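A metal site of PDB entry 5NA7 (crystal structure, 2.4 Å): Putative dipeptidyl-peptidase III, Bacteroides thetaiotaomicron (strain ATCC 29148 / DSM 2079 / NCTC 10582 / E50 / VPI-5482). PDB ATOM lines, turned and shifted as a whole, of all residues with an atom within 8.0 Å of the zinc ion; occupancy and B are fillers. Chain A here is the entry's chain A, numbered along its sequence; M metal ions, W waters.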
ATOM      1  N   THR A 445      -3.077 -23.590  24.817  1.00  0.00           N
ATOM      2  CA  THR A 445      -1.776 -22.932  24.726  1.00  0.00           C
ATOM      3  C   THR A 445      -1.671 -22.094  23.463  1.00  0.00           C
ATOM      4  O   THR A 445      -1.227 -20.949  23.499  1.00  0.00           O
ATOM      5  CB  THR A 445      -0.668 -23.989  24.773  1.00  0.00           C
ATOM      6  OG1 THR A 445      -0.736 -24.703  26.008  1.00  0.00           O
ATOM      7  CG2 THR A 445       0.718 -23.326  24.605  1.00  0.00           C
ATOM      8  N   HIS A 448      -3.758 -18.969  23.853  1.00  0.00           N
ATOM      9  CA  HIS A 448      -3.062 -18.062  24.766  1.00  0.00           C
ATOM     10  C   HIS A 448      -1.900 -17.379  24.042  1.00  0.00           C
ATOM     11  O   HIS A 448      -1.779 -16.146  24.059  1.00  0.00           O
ATOM     12  CB  HIS A 448      -2.616 -18.842  26.015  1.00  0.00           C
ATOM     13  CG  HIS A 448      -1.648 -18.128  26.917  1.00  0.00           C
ATOM     14  ND1 HIS A 448      -1.745 -18.198  28.281  1.00  0.00           N
ATOM     15  CD2 HIS A 448      -0.523 -17.421  26.654  1.00  0.00           C
ATOM     16  CE1 HIS A 448      -0.752 -17.515  28.832  1.00  0.00           C
ATOM     17  NE2 HIS A 448       0.004 -17.043  27.867  1.00  0.00           N
ATOM     18  N   GLU A 449      -1.019 -18.163  23.413  1.00  0.00           N
ATOM     19  CA  GLU A 449       0.210 -17.611  22.845  1.00  0.00           C
ATOM     20  C   GLU A 449      -0.049 -16.863  21.537  1.00  0.00           C
ATOM     21  O   GLU A 449       0.564 -15.816  21.292  1.00  0.00           O
ATOM     22  CB  GLU A 449       1.217 -18.733  22.613  1.00  0.00           C
ATOM     23  CG  GLU A 449       1.805 -19.309  23.888  1.00  0.00           C
ATOM     24  CD  GLU A 449       2.803 -20.415  23.613  1.00  0.00           C
ATOM     25  OE1 GLU A 449       3.048 -20.710  22.420  1.00  0.00           O
ATOM     26  OE2 GLU A 449       3.359 -20.976  24.576  1.00  0.00           O
ATOM     27  N   CYS A 450      -0.936 -17.367  20.680  1.00  0.00           N
ATOM     28  CA  CYS A 450      -1.151 -16.728  19.392  1.00  0.00           C
ATOM     29  C   CYS A 450      -2.102 -15.547  19.462  1.00  0.00           C
ATOM     30  O   CYS A 450      -1.976 -14.611  18.671  1.00  0.00           O
ATOM     31  CB  CYS A 450      -1.678 -17.738  18.361  1.00  0.00           C
ATOM     32  SG  CYS A 450      -0.596 -19.158  18.071  1.00  0.00           S
ATOM     33  N   GLY A 452      -4.084 -14.575  22.810  1.00  0.00           N
ATOM     34  CA  GLY A 452      -4.481 -14.061  24.116  1.00  0.00           C
ATOM     35  C   GLY A 452      -3.743 -12.792  24.511  1.00  0.00           C
ATOM     36  O   GLY A 452      -4.347 -11.790  24.886  1.00  0.00           O
ATOM     37  N   HIS A 453      -2.404 -12.817  24.392  1.00  0.00           N
ATOM     38  CA  HIS A 453      -1.626 -11.627  24.747  1.00  0.00           C
ATOM     39  C   HIS A 453      -1.849 -10.487  23.754  1.00  0.00           C
ATOM     40  O   HIS A 453      -1.876  -9.316  24.143  1.00  0.00           O
ATOM     41  CB  HIS A 453      -0.133 -11.980  24.806  1.00  0.00           C
ATOM     42  CG  HIS A 453       0.252 -12.815  25.993  1.00  0.00           C
ATOM     43  ND1 HIS A 453       0.119 -12.370  27.289  1.00  0.00           N
ATOM     44  CD2 HIS A 453       0.778 -14.052  26.074  1.00  0.00           C
ATOM     45  CE1 HIS A 453       0.542 -13.314  28.120  1.00  0.00           C
ATOM     46  NE2 HIS A 453       0.946 -14.341  27.410  1.00  0.00           N
ATOM     47  N   SER A 472       2.314  -8.975  35.750  1.00  0.00           N
ATOM     48  CA  SER A 472       2.624 -10.247  35.121  1.00  0.00           C
ATOM     49  C   SER A 472       1.553 -11.303  35.425  1.00  0.00           C
ATOM     50  O   SER A 472       1.128 -12.032  34.527  1.00  0.00           O
ATOM     51  CB  SER A 472       3.998 -10.724  35.578  1.00  0.00           C
ATOM     52  OG  SER A 472       4.381 -11.923  34.918  1.00  0.00           O
ATOM     53  N   GLU A 475      -1.674 -10.346  33.521  1.00  0.00           N
ATOM     54  CA  GLU A 475      -1.545 -10.508  32.076  1.00  0.00           C
ATOM     55  C   GLU A 475      -1.594 -11.966  31.656  1.00  0.00           C
ATOM     56  O   GLU A 475      -2.206 -12.314  30.644  1.00  0.00           O
ATOM     57  CB  GLU A 475      -0.246  -9.855  31.594  1.00  0.00           C
ATOM     58  CG  GLU A 475       0.047 -10.012  30.098  1.00  0.00           C
ATOM     59  CD  GLU A 475      -1.053  -9.502  29.185  1.00  0.00           C
ATOM     60  OE1 GLU A 475      -1.141  -9.996  28.039  1.00  0.00           O
ATOM     61  OE2 GLU A 475      -1.838  -8.615  29.594  1.00  0.00           O
ATOM     62  N   GLU A 476      -0.933 -12.841  32.416  1.00  0.00           N
ATOM     63  CA  GLU A 476      -1.018 -14.249  32.096  1.00  0.00           C
ATOM     64  C   GLU A 476      -2.416 -14.817  32.348  1.00  0.00           C
ATOM     65  O   GLU A 476      -2.912 -15.635  31.574  1.00  0.00           O
ATOM     66  CB  GLU A 476       0.037 -15.005  32.897  1.00  0.00           C
ATOM     67  CG  GLU A 476       0.890 -15.897  32.034  1.00  0.00           C
ATOM     68  CD  GLU A 476       1.551 -15.149  30.908  1.00  0.00           C
ATOM     69  OE1 GLU A 476       2.398 -14.273  31.179  1.00  0.00           O
ATOM     70  OE2 GLU A 476       1.221 -15.431  29.751  1.00  0.00           O
ATOM     71  N   ALA A 477      -3.081 -14.381  33.419  1.00  0.00           N
ATOM     72  CA  ALA A 477      -4.481 -14.743  33.616  1.00  0.00           C
ATOM     73  C   ALA A 477      -5.352 -14.310  32.440  1.00  0.00           C
ATOM     74  O   ALA A 477      -6.199 -15.082  31.963  1.00  0.00           O
ATOM     75  CB  ALA A 477      -5.004 -14.134  34.921  1.00  0.00           C
ATOM     76  N   ALA A 479      -4.544 -13.850  29.238  1.00  0.00           N
ATOM     77  CA  ALA A 479      -4.314 -14.681  28.074  1.00  0.00           C
ATOM     78  C   ALA A 479      -4.882 -16.084  28.294  1.00  0.00           C
ATOM     79  O   ALA A 479      -5.467 -16.673  27.372  1.00  0.00           O
ATOM     80  CB  ALA A 479      -2.813 -14.745  27.761  1.00  0.00           C
ATOM     81  N   ASP A 480      -4.724 -16.638  29.499  1.00  0.00           N
ATOM     82  CA  ASP A 480      -5.291 -17.951  29.799  1.00  0.00           C
ATOM     83  C   ASP A 480      -6.805 -17.947  29.675  1.00  0.00           C
ATOM     84  O   ASP A 480      -7.388 -18.898  29.131  1.00  0.00           O
ATOM     85  CB  ASP A 480      -4.902 -18.389  31.208  1.00  0.00           C
ATOM     86  CG  ASP A 480      -3.696 -19.304  31.231  1.00  0.00           C
ATOM     87  OD1 ASP A 480      -3.142 -19.578  30.145  1.00  0.00           O
ATOM     88  OD2 ASP A 480      -3.356 -19.784  32.333  1.00  0.00           O
ATOM     89  N   HIS A 533       2.733 -17.504  37.037  1.00  0.00           N
ATOM     90  CA  HIS A 533       1.852 -18.411  36.310  1.00  0.00           C
ATOM     91  C   HIS A 533       1.048 -19.295  37.259  1.00  0.00           C
ATOM     92  O   HIS A 533      -0.159 -19.510  37.047  1.00  0.00           O
ATOM     93  CB  HIS A 533       2.642 -19.278  35.335  1.00  0.00           C
ATOM     94  CG  HIS A 533       3.183 -18.519  34.165  1.00  0.00           C
ATOM     95  ND1 HIS A 533       4.344 -17.776  34.223  1.00  0.00           N
ATOM     96  CD2 HIS A 533       2.721 -18.396  32.896  1.00  0.00           C
ATOM     97  CE1 HIS A 533       4.572 -17.233  33.042  1.00  0.00           C
ATOM     98  NE2 HIS A 533       3.601 -17.589  32.215  1.00  0.00           N
ATOM     99  N   ASN A 536      -1.669 -17.176  38.531  1.00  0.00           N
ATOM    100  CA  ASN A 536      -2.743 -16.831  37.614  1.00  0.00           C
ATOM    101  C   ASN A 536      -3.700 -18.004  37.471  1.00  0.00           C
ATOM    102  O   ASN A 536      -4.901 -17.806  37.269  1.00  0.00           O
ATOM    103  CB  ASN A 536      -2.166 -16.338  36.269  1.00  0.00           C
ATOM    104  CG  ASN A 536      -2.159 -17.403  35.163  1.00  0.00           C
ATOM    105  OD1 ASN A 536      -1.097 -17.763  34.656  1.00  0.00           O
ATOM    106  ND2 ASN A 536      -3.339 -17.809  34.702  1.00  0.00           N
HETATM  107 ZN    ZN M   1       1.816 -16.089  28.018  1.00  0.00          ZN
HETATM  108  O   HOH W   1       2.678 -17.874  28.797  1.00  0.00           O
HETATM  109  O   HOH W   2       3.605 -15.043  28.408  1.00  0.00           O
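ND1 of His 453 is in hydrogen-bond range of OE1 of Glu 475, 2.8 Å away.
A ring nitrogen (ND1) of His 448 lies within hydrogen-bond range of the side-chain carboxylate (OD1) of Asp 480 (2.7 Å).
The zinc ion is bound by OE2 of Glu 476 (1.9 Å).
NE2 of His 453 binds the zinc ion, at 2.0 Å.
NE2 of His 448 is bound to the zinc ion (2.1 Å).
Water W2 binds the zinc ion (2.1 Å).
Water W1 binds the zinc ion (2.1 Å).
The nearest printed residue that does not touch the zinc ion is His 533 (4.8 Å).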
